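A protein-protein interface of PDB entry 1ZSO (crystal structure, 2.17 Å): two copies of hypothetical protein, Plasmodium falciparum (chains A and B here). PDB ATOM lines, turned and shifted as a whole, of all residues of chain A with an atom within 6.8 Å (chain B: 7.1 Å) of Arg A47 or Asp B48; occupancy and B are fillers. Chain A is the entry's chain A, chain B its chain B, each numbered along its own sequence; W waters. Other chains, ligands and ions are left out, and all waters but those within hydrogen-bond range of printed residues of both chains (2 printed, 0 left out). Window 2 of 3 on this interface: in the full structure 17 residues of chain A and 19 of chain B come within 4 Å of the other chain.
Arg A47 touches its own counterpart, Arg B47. Arg A47 touches Asp B48, and with the chains exchanged Asp A48 touches Arg B47. Arg A47 touches Asn B49, and with the chains exchanged Asn A49 touches Arg B47. Ile A50 touches Arg B47, but with the chains exchanged Arg A47 does not touch Ile B50 (4.1 Å). Positions printed for both chains: 36, 37, 38, 46, 47, 48, 49, 50 and 69. Of the 7 pairs that touch across the chains among the printed residues, 5 have their exchanged pair printed and touching as well.
The guanidinium group (NH1) of Arg A47 lies within hydrogen-bond range of the backbone carbonyl oxygen (O) of Asp B48. The guanidinium group of Arg A47 is in hydrogen-bond range of the backbone carbonyl oxygen of Asn B49. O of Asp A48 sits at hydrogen-bond distance from NH1 of Arg B47 (2.6 Å). NH2 of Arg B47 lies within hydrogen-bond range of O of Asn A49 (3.0 Å). NH2 of Arg A47 sits close to NE of Arg B47 (3.5 Å).
The backbone carbonyl oxygen of Phe A36 is in hydrogen-bond range of the backbone NH of Asn A49 (3.1 Å). The side-chain amide oxygen (OD1) of Asn A37 sits at hydrogen-bond distance from the backbone NH (N) of Asn A49. The backbone NH of Ile A38 is in hydrogen-bond range of the backbone carbonyl oxygen of Arg A47 (2.7 Å). O of Phe B36 sits at hydrogen-bond distance from N of Asn B49 (3.0 Å). N of Asn B49 sits at hydrogen-bond distance from OD1 of Asn B37, 3.0 Å away. The backbone carbonyl oxygen (O) of Arg B47 is in hydrogen-bond range of the backbone NH (N) of Ile B38 (2.9 Å).
Among the printed residues, merely in contact across the chains: Ile A50 with Arg B47 (3.6 Å) and Ile A71 with Gln B51 (3.7 Å).
Of chain B, only Arg B47, Asp B48 and Asn B49 come within 4 Å of Arg A47. Asp B48 touches just one residue of chain A: Arg A47 (2.9 Å). Of the printed residues of chain B, Ile A71 touches Gln B51. Of the printed residues of chain A, Asn B49 touches Arg A47. Of the printed residues of chain B, Asp A48 touches Arg B47 (2.6 Å). Printed residues of chain A within 4 Å of Gln B51: Ile A71. Of the printed residues of chain B, Asn A49 touches Arg B47 (3.0 Å). Leu A45 touches none of the printed residues of chain B. Asp B116 touches none of the printed residues of chain A. The nearest printed residue of chain B that does not touch Asn A49 is Phe B69 (7.9 Å).
Printed residues of chain A that touch a printed residue of chain B: Arg A47, Asp A48, Asn A49, Ile A50 and Ile A71. Hydrophobic or aromatic side chains of chain A within 4 Å of the printed part of chain B: Ile A71. Among the printed residues, 7 pairs touch across the chains. Among the printed residues, no Asp or Glu carboxylate lies within 4 Å of a Lys or Arg side-chain nitrogen of the other chain.
Water W1 lies within hydrogen-bond range of O of Asn B49 (2.5 Å) and NE of Arg A47 (3.5 Å). Water W2 lies within hydrogen-bond range of NH2 of Arg B47 (3.3 Å) and NH2 of Arg A47 (3.3 Å).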
ATOM      1  N   PHE A  36       9.013  32.848  15.370  1.00  0.00           N
ATOM      2  CA  PHE A  36       8.166  32.478  14.220  1.00  0.00           C
ATOM      3  C   PHE A  36       8.536  31.143  13.587  1.00  0.00           C
ATOM      4  O   PHE A  36       9.676  30.710  13.686  1.00  0.00           O
ATOM      5  CB  PHE A  36       8.273  33.541  13.102  1.00  0.00           C
ATOM      6  CG  PHE A  36       7.716  34.909  13.465  1.00  0.00           C
ATOM      7  CD1 PHE A  36       6.357  35.164  13.414  1.00  0.00           C
ATOM      8  CD2 PHE A  36       8.564  35.957  13.787  1.00  0.00           C
ATOM      9  CE1 PHE A  36       5.853  36.430  13.717  1.00  0.00           C
ATOM     10  CE2 PHE A  36       8.071  37.205  14.096  1.00  0.00           C
ATOM     11  CZ  PHE A  36       6.693  37.445  14.052  1.00  0.00           C
ATOM     12  N   ASN A  37       7.553  30.524  12.929  1.00  0.00           N
ATOM     13  CA  ASN A  37       7.777  29.549  11.845  1.00  0.00           C
ATOM     14  C   ASN A  37       7.578  30.277  10.551  1.00  0.00           C
ATOM     15  O   ASN A  37       6.634  31.055  10.417  1.00  0.00           O
ATOM     16  CB  ASN A  37       6.763  28.425  11.877  1.00  0.00           C
ATOM     17  CG  ASN A  37       6.857  27.613  13.107  1.00  0.00           C
ATOM     18  OD1 ASN A  37       7.882  27.594  13.765  1.00  0.00           O
ATOM     19  ND2 ASN A  37       5.769  26.930  13.446  1.00  0.00           N
ATOM     20  N   ILE A  38       8.458  30.022   9.596  1.00  0.00           N
ATOM     21  CA  ILE A  38       8.463  30.757   8.369  1.00  0.00           C
ATOM     22  C   ILE A  38       8.580  29.806   7.181  1.00  0.00           C
ATOM     23  O   ILE A  38       8.898  28.610   7.325  1.00  0.00           O
ATOM     24  CB  ILE A  38       9.629  31.795   8.347  1.00  0.00           C
ATOM     25  CG1 ILE A  38      11.012  31.095   8.271  1.00  0.00           C
ATOM     26  CG2 ILE A  38       9.594  32.674   9.616  1.00  0.00           C
ATOM     27  CD1 ILE A  38      12.232  32.014   8.063  1.00  0.00           C
ATOM     28  N   ARG A  39       8.350  30.377   6.015  1.00  0.00           N
ATOM     29  CA  ARG A  39       8.306  29.670   4.776  1.00  0.00           C
ATOM     30  C   ARG A  39       8.941  30.538   3.687  1.00  0.00           C
ATOM     31  O   ARG A  39       8.817  31.749   3.703  1.00  0.00           O
ATOM     32  CB  ARG A  39       6.859  29.394   4.384  1.00  0.00           C
ATOM     33  CG  ARG A  39       6.749  28.805   3.013  1.00  0.00           C
ATOM     34  CD  ARG A  39       5.566  27.946   2.847  1.00  0.00           C
ATOM     35  NE  ARG A  39       4.388  28.704   2.454  1.00  0.00           N
ATOM     36  CZ  ARG A  39       3.233  28.714   3.129  1.00  0.00           C
ATOM     37  NH1 ARG A  39       3.087  28.004   4.263  1.00  0.00           N
ATOM     38  NH2 ARG A  39       2.207  29.433   2.664  1.00  0.00           N
ATOM     39  N   ASP A  40       9.602  29.892   2.736  1.00  0.00           N
ATOM     40  CA  ASP A  40      10.148  30.533   1.568  1.00  0.00           C
ATOM     41  C   ASP A  40       8.968  31.063   0.783  1.00  0.00           C
ATOM     42  O   ASP A  40       7.987  30.348   0.602  1.00  0.00           O
ATOM     43  CB  ASP A  40      10.887  29.461   0.781  1.00  0.00           C
ATOM     44  CG  ASP A  40      11.596  29.980  -0.444  1.00  0.00           C
ATOM     45  OD1 ASP A  40      11.289  31.081  -0.910  1.00  0.00           O
ATOM     46  OD2 ASP A  40      12.479  29.247  -0.945  1.00  0.00           O
ATOM     47  N   LEU A  45       9.931  25.224   1.035  1.00  0.00           N
ATOM     48  CA  LEU A  45      10.848  25.195   2.177  1.00  0.00           C
ATOM     49  C   LEU A  45      10.351  25.990   3.383  1.00  0.00           C
ATOM     50  O   LEU A  45       9.812  27.065   3.250  1.00  0.00           O
ATOM     51  CB  LEU A  45      12.207  25.764   1.767  1.00  0.00           C
ATOM     52  CG  LEU A  45      13.003  24.989   0.721  1.00  0.00           C
ATOM     53  CD1 LEU A  45      14.267  25.760   0.356  1.00  0.00           C
ATOM     54  CD2 LEU A  45      13.385  23.641   1.274  1.00  0.00           C
ATOM     55  N   THR A  46      10.563  25.456   4.569  1.00  0.00           N
ATOM     56  CA  THR A  46      10.163  26.138   5.761  1.00  0.00           C
ATOM     57  C   THR A  46      11.271  26.078   6.789  1.00  0.00           C
ATOM     58  O   THR A  46      12.205  25.283   6.677  1.00  0.00           O
ATOM     59  CB  THR A  46       8.883  25.530   6.390  1.00  0.00           C
ATOM     60  OG1 THR A  46       9.135  24.204   6.855  1.00  0.00           O
ATOM     61  CG2 THR A  46       7.755  25.507   5.431  1.00  0.00           C
ATOM     62  N   ARG A  47      11.151  26.934   7.795  1.00  0.00           N
ATOM     63  CA  ARG A  47      12.048  26.919   8.920  1.00  0.00           C
ATOM     64  C   ARG A  47      11.206  27.273  10.140  1.00  0.00           C
ATOM     65  O   ARG A  47      10.475  28.278  10.146  1.00  0.00           O
ATOM     66  CB  ARG A  47      13.147  27.960   8.689  1.00  0.00           C
ATOM     67  CG  ARG A  47      14.241  27.993   9.696  1.00  0.00           C
ATOM     68  CD  ARG A  47      15.339  27.118   9.384  1.00  0.00           C
ATOM     69  NE  ARG A  47      16.419  27.282  10.376  1.00  0.00           N
ATOM     70  CZ  ARG A  47      17.261  26.309  10.711  1.00  0.00           C
ATOM     71  NH1 ARG A  47      17.124  25.124  10.186  1.00  0.00           N
ATOM     72  NH2 ARG A  47      18.211  26.501  11.600  1.00  0.00           N
ATOM     73  N   ASP A  48      11.282  26.421  11.135  1.00  0.00           N
ATOM     74  CA  ASP A  48      10.520  26.579  12.382  1.00  0.00           C
ATOM     75  C   ASP A  48      11.380  27.188  13.431  1.00  0.00           C
ATOM     76  O   ASP A  48      12.619  27.030  13.404  1.00  0.00           O
ATOM     77  CB  ASP A  48      10.023  25.223  12.919  1.00  0.00           C
ATOM     78  CG  ASP A  48       9.016  24.559  12.002  1.00  0.00           C
ATOM     79  OD1 ASP A  48       8.651  25.138  10.979  1.00  0.00           O
ATOM     80  OD2 ASP A  48       8.509  23.484  12.348  1.00  0.00           O
ATOM     81  N   ASN A  49      10.711  27.902  14.336  1.00  0.00           N
ATOM     82  CA  ASN A  49      11.316  28.418  15.542  1.00  0.00           C
ATOM     83  C   ASN A  49      12.562  29.306  15.272  1.00  0.00           C
ATOM     84  O   ASN A  49      13.553  29.205  15.967  1.00  0.00           O
ATOM     85  CB  ASN A  49      11.640  27.240  16.493  1.00  0.00           C
ATOM     86  CG  ASN A  49      11.833  27.675  17.962  1.00  0.00           C
ATOM     87  OD1 ASN A  49      11.435  28.759  18.377  1.00  0.00           O
ATOM     88  ND2 ASN A  49      12.429  26.792  18.761  1.00  0.00           N
ATOM     89  N   ILE A  50      12.497  30.202  14.287  1.00  0.00           N
ATOM     90  CA  ILE A  50      13.532  31.245  14.154  1.00  0.00           C
ATOM     91  C   ILE A  50      13.265  32.256  15.275  1.00  0.00           C
ATOM     92  O   ILE A  50      12.102  32.393  15.729  1.00  0.00           O
ATOM     93  CB  ILE A  50      13.491  31.980  12.812  1.00  0.00           C
ATOM     94  CG1 ILE A  50      12.105  32.592  12.582  1.00  0.00           C
ATOM     95  CG2 ILE A  50      13.713  30.989  11.667  1.00  0.00           C
ATOM     96  CD1 ILE A  50      12.054  34.000  12.041  1.00  0.00           C
ATOM     97  N   PHE A  69      16.673  39.521  10.843  1.00  0.00           N
ATOM     98  CA  PHE A  69      16.795  38.096  10.543  1.00  0.00           C
ATOM     99  C   PHE A  69      17.047  37.870   9.062  1.00  0.00           C
ATOM    100  O   PHE A  69      16.461  38.538   8.202  1.00  0.00           O
ATOM    101  CB  PHE A  69      15.548  37.318  10.984  1.00  0.00           C
ATOM    102  CG  PHE A  69      15.610  35.860  10.648  1.00  0.00           C
ATOM    103  CD1 PHE A  69      16.179  34.955  11.533  1.00  0.00           C
ATOM    104  CD2 PHE A  69      15.143  35.402   9.427  1.00  0.00           C
ATOM    105  CE1 PHE A  69      16.251  33.592  11.215  1.00  0.00           C
ATOM    106  CE2 PHE A  69      15.193  34.057   9.100  1.00  0.00           C
ATOM    107  CZ  PHE A  69      15.765  33.141  10.010  1.00  0.00           C
ATOM    108  N   ILE A  71      18.087  34.582   6.016  1.00  0.00           N
ATOM    109  CA  ILE A  71      18.309  33.216   5.669  1.00  0.00           C
ATOM    110  C   ILE A  71      18.616  33.147   4.190  1.00  0.00           C
ATOM    111  O   ILE A  71      18.087  33.915   3.419  1.00  0.00           O
ATOM    112  CB  ILE A  71      17.082  32.349   6.091  1.00  0.00           C
ATOM    113  CG1 ILE A  71      17.414  30.866   5.920  1.00  0.00           C
ATOM    114  CG2 ILE A  71      15.833  32.744   5.316  1.00  0.00           C
ATOM    115  CD1 ILE A  71      16.285  29.936   6.290  1.00  0.00           C
ATOM    116  N   TRP A  73      18.033  30.459   1.607  1.00  0.00           N
ATOM    117  CA  TRP A  73      17.223  29.228   1.545  1.00  0.00           C
ATOM    118  C   TRP A  73      17.862  28.067   0.768  1.00  0.00           C
ATOM    119  O   TRP A  73      17.626  26.902   1.094  1.00  0.00           O
ATOM    120  CB  TRP A  73      15.852  29.499   0.958  1.00  0.00           C
ATOM    121  CG  TRP A  73      14.882  30.226   1.812  1.00  0.00           C
ATOM    122  CD1 TRP A  73      14.411  31.481   1.586  1.00  0.00           C
ATOM    123  CD2 TRP A  73      14.159  29.724   2.939  1.00  0.00           C
ATOM    124  NE1 TRP A  73      13.469  31.820   2.529  1.00  0.00           N
ATOM    125  CE2 TRP A  73      13.286  30.750   3.363  1.00  0.00           C
ATOM    126  CE3 TRP A  73      14.125  28.491   3.606  1.00  0.00           C
ATOM    127  CZ2 TRP A  73      12.441  30.607   4.466  1.00  0.00           C
ATOM    128  CZ3 TRP A  73      13.303  28.351   4.687  1.00  0.00           C
ATOM    129  CH2 TRP A  73      12.460  29.389   5.108  1.00  0.00           C
ATOM    130  N   ILE B  35      27.984  27.869   8.572  1.00  0.00           N
ATOM    131  CA  ILE B  35      26.864  26.906   8.566  1.00  0.00           C
ATOM    132  C   ILE B  35      27.239  25.717   9.460  1.00  0.00           C
ATOM    133  O   ILE B  35      28.339  25.132   9.387  1.00  0.00           O
ATOM    134  CB  ILE B  35      26.526  26.475   7.146  1.00  0.00           C
ATOM    135  CG1 ILE B  35      26.296  27.720   6.279  1.00  0.00           C
ATOM    136  CG2 ILE B  35      25.266  25.595   7.111  1.00  0.00           C
ATOM    137  CD1 ILE B  35      26.275  27.455   4.829  1.00  0.00           C
ATOM    138  N   PHE B  36      26.360  25.386  10.372  1.00  0.00           N
ATOM    139  CA  PHE B  36      26.663  24.313  11.322  1.00  0.00           C
ATOM    140  C   PHE B  36      25.407  23.573  11.621  1.00  0.00           C
ATOM    141  O   PHE B  36      24.300  24.135  11.541  1.00  0.00           O
ATOM    142  CB  PHE B  36      27.199  24.882  12.636  1.00  0.00           C
ATOM    143  CG  PHE B  36      28.600  25.433  12.537  1.00  0.00           C
ATOM    144  CD1 PHE B  36      29.676  24.586  12.539  1.00  0.00           C
ATOM    145  CD2 PHE B  36      28.820  26.794  12.454  1.00  0.00           C
ATOM    146  CE1 PHE B  36      30.986  25.087  12.430  1.00  0.00           C
ATOM    147  CE2 PHE B  36      30.100  27.302  12.349  1.00  0.00           C
ATOM    148  CZ  PHE B  36      31.188  26.443  12.344  1.00  0.00           C
ATOM    149  N   ASN B  37      25.587  22.304  11.963  1.00  0.00           N
ATOM    150  CA  ASN B  37      24.645  21.652  12.809  1.00  0.00           C
ATOM    151  C   ASN B  37      25.123  21.751  14.261  1.00  0.00           C
ATOM    152  O   ASN B  37      26.276  21.457  14.589  1.00  0.00           O
ATOM    153  CB  ASN B  37      24.489  20.188  12.466  1.00  0.00           C
ATOM    154  CG  ASN B  37      23.921  19.931  11.091  1.00  0.00           C
ATOM    155  OD1 ASN B  37      23.249  20.752  10.468  1.00  0.00           O
ATOM    156  ND2 ASN B  37      24.162  18.713  10.627  1.00  0.00           N
ATOM    157  N   ILE B  38      24.203  22.156  15.129  1.00  0.00           N
ATOM    158  CA  ILE B  38      24.480  22.305  16.554  1.00  0.00           C
ATOM    159  C   ILE B  38      23.593  21.456  17.463  1.00  0.00           C
ATOM    160  O   ILE B  38      22.573  20.888  17.045  1.00  0.00           O
ATOM    161  CB  ILE B  38      24.343  23.765  16.968  1.00  0.00           C
ATOM    162  CG1 ILE B  38      22.881  24.199  16.816  1.00  0.00           C
ATOM    163  CG2 ILE B  38      25.337  24.626  16.107  1.00  0.00           C
ATOM    164  CD1 ILE B  38      22.497  25.474  17.589  1.00  0.00           C
ATOM    165  N   THR B  46      18.675  19.672  19.148  1.00  0.00           N
ATOM    166  CA  THR B  46      19.615  19.943  18.063  1.00  0.00           C
ATOM    167  C   THR B  46      18.975  20.950  17.118  1.00  0.00           C
ATOM    168  O   THR B  46      17.767  21.112  17.100  1.00  0.00           O
ATOM    169  CB  THR B  46      19.948  18.666  17.279  1.00  0.00           C
ATOM    170  OG1 THR B  46      18.743  18.111  16.724  1.00  0.00           O
ATOM    171  CG2 THR B  46      20.534  17.648  18.157  1.00  0.00           C
ATOM    172  N   ARG B  47      19.801  21.636  16.339  1.00  0.00           N
ATOM    173  CA  ARG B  47      19.324  22.538  15.304  1.00  0.00           C
ATOM    174  C   ARG B  47      20.256  22.386  14.089  1.00  0.00           C
ATOM    175  O   ARG B  47      21.467  22.522  14.235  1.00  0.00           O
ATOM    176  CB  ARG B  47      19.336  23.945  15.876  1.00  0.00           C
ATOM    177  CG  ARG B  47      18.744  25.010  15.021  1.00  0.00           C
ATOM    178  CD  ARG B  47      17.206  25.077  15.166  1.00  0.00           C
ATOM    179  NE  ARG B  47      16.751  26.413  14.778  1.00  0.00           N
ATOM    180  CZ  ARG B  47      15.587  26.677  14.198  1.00  0.00           C
ATOM    181  NH1 ARG B  47      14.732  25.690  13.897  1.00  0.00           N
ATOM    182  NH2 ARG B  47      15.299  27.940  13.888  1.00  0.00           N
ATOM    183  N   ASP B  48      19.702  22.040  12.926  1.00  0.00           N
ATOM    184  CA  ASP B  48      20.496  21.870  11.708  1.00  0.00           C
ATOM    185  C   ASP B  48      20.597  23.155  10.918  1.00  0.00           C
ATOM    186  O   ASP B  48      19.653  23.939  10.877  1.00  0.00           O
ATOM    187  CB  ASP B  48      19.873  20.849  10.757  1.00  0.00           C
ATOM    188  CG  ASP B  48      19.954  19.428  11.281  1.00  0.00           C
ATOM    189  OD1 ASP B  48      20.574  19.229  12.352  1.00  0.00           O
ATOM    190  OD2 ASP B  48      19.361  18.522  10.621  1.00  0.00           O
ATOM    191  N   ASN B  49      21.741  23.344  10.275  1.00  0.00           N
ATOM    192  CA  ASN B  49      21.880  24.381   9.252  1.00  0.00           C
ATOM    193  C   ASN B  49      21.611  25.761   9.816  1.00  0.00           C
ATOM    194  O   ASN B  49      20.789  26.514   9.273  1.00  0.00           O
ATOM    195  CB  ASN B  49      20.894  24.102   8.115  1.00  0.00           C
ATOM    196  CG  ASN B  49      21.124  25.020   6.880  1.00  0.00           C
ATOM    197  OD1 ASN B  49      22.256  25.194   6.404  1.00  0.00           O
ATOM    198  ND2 ASN B  49      20.034  25.592   6.359  1.00  0.00           N
ATOM    199  N   ILE B  50      22.248  26.086  10.938  1.00  0.00           N
ATOM    200  CA  ILE B  50      22.183  27.431  11.391  1.00  0.00           C
ATOM    201  C   ILE B  50      23.150  28.155  10.516  1.00  0.00           C
ATOM    202  O   ILE B  50      24.137  27.556  10.014  1.00  0.00           O
ATOM    203  CB  ILE B  50      22.567  27.627  12.862  1.00  0.00           C
ATOM    204  CG1 ILE B  50      24.031  27.248  13.113  1.00  0.00           C
ATOM    205  CG2 ILE B  50      21.641  26.849  13.733  1.00  0.00           C
ATOM    206  CD1 ILE B  50      24.579  27.886  14.284  1.00  0.00           C
ATOM    207  N   GLN B  51      22.876  29.436  10.327  1.00  0.00           N
ATOM    208  CA  GLN B  51      23.698  30.260   9.445  1.00  0.00           C
ATOM    209  C   GLN B  51      24.054  31.603  10.117  1.00  0.00           C
ATOM    210  O   GLN B  51      23.221  32.297  10.737  1.00  0.00           O
ATOM    211  CB  GLN B  51      22.984  30.514   8.105  1.00  0.00           C
ATOM    212  CG  GLN B  51      22.376  29.305   7.415  1.00  0.00           C
ATOM    213  CD  GLN B  51      21.572  29.696   6.197  1.00  0.00           C
ATOM    214  OE1 GLN B  51      21.107  30.810   6.103  1.00  0.00           O
ATOM    215  NE2 GLN B  51      21.426  28.786   5.249  1.00  0.00           N
ATOM    216  N   PHE B  69      25.710  34.512  16.791  1.00  0.00           N
ATOM    217  CA  PHE B  69      24.555  33.615  16.804  1.00  0.00           C
ATOM    218  C   PHE B  69      24.054  33.363  18.219  1.00  0.00           C
ATOM    219  O   PHE B  69      24.845  33.169  19.145  1.00  0.00           O
ATOM    220  CB  PHE B  69      24.874  32.251  16.160  1.00  0.00           C
ATOM    221  CG  PHE B  69      23.678  31.335  16.074  1.00  0.00           C
ATOM    222  CD1 PHE B  69      22.770  31.455  15.035  1.00  0.00           C
ATOM    223  CD2 PHE B  69      23.426  30.389  17.055  1.00  0.00           C
ATOM    224  CE1 PHE B  69      21.609  30.591  14.961  1.00  0.00           C
ATOM    225  CE2 PHE B  69      22.316  29.561  16.977  1.00  0.00           C
ATOM    226  CZ  PHE B  69      21.391  29.677  15.915  1.00  0.00           C
ATOM    227  N   ASP B 116      28.564  19.581  13.282  1.00  0.00           N
ATOM    228  CA  ASP B 116      28.916  19.407  11.892  1.00  0.00           C
ATOM    229  C   ASP B 116      29.100  20.783  11.291  1.00  0.00           C
ATOM    230  O   ASP B 116      28.291  21.644  11.516  1.00  0.00           O
ATOM    231  CB  ASP B 116      27.774  18.733  11.125  1.00  0.00           C
ATOM    232  CG  ASP B 116      27.473  17.338  11.618  1.00  0.00           C
ATOM    233  OD1 ASP B 116      28.431  16.541  11.773  1.00  0.00           O
ATOM    234  OD2 ASP B 116      26.267  17.019  11.825  1.00  0.00           O
ATOM    235  N   PHE B 118      29.645  22.878   7.592  1.00  0.00           N
ATOM    236  CA  PHE B 118      29.358  22.811   6.188  1.00  0.00           C
ATOM    237  C   PHE B 118      30.020  23.946   5.457  1.00  0.00           C
ATOM    238  O   PHE B 118      29.562  25.041   5.521  1.00  0.00           O
ATOM    239  CB  PHE B 118      27.864  22.862   5.944  1.00  0.00           C
ATOM    240  CG  PHE B 118      27.147  21.734   6.572  1.00  0.00           C
ATOM    241  CD1 PHE B 118      26.801  21.788   7.909  1.00  0.00           C
ATOM    242  CD2 PHE B 118      26.866  20.582   5.849  1.00  0.00           C
ATOM    243  CE1 PHE B 118      26.158  20.713   8.519  1.00  0.00           C
ATOM    244  CE2 PHE B 118      26.215  19.517   6.445  1.00  0.00           C
ATOM    245  CZ  PHE B 118      25.885  19.588   7.805  1.00  0.00           C
HETATM  246  O   HOH W   1      18.970  27.798   8.059  1.00  0.00           O
HETATM  247  O   HOH W   2      17.857  29.599  12.722  1.00  0.00           O
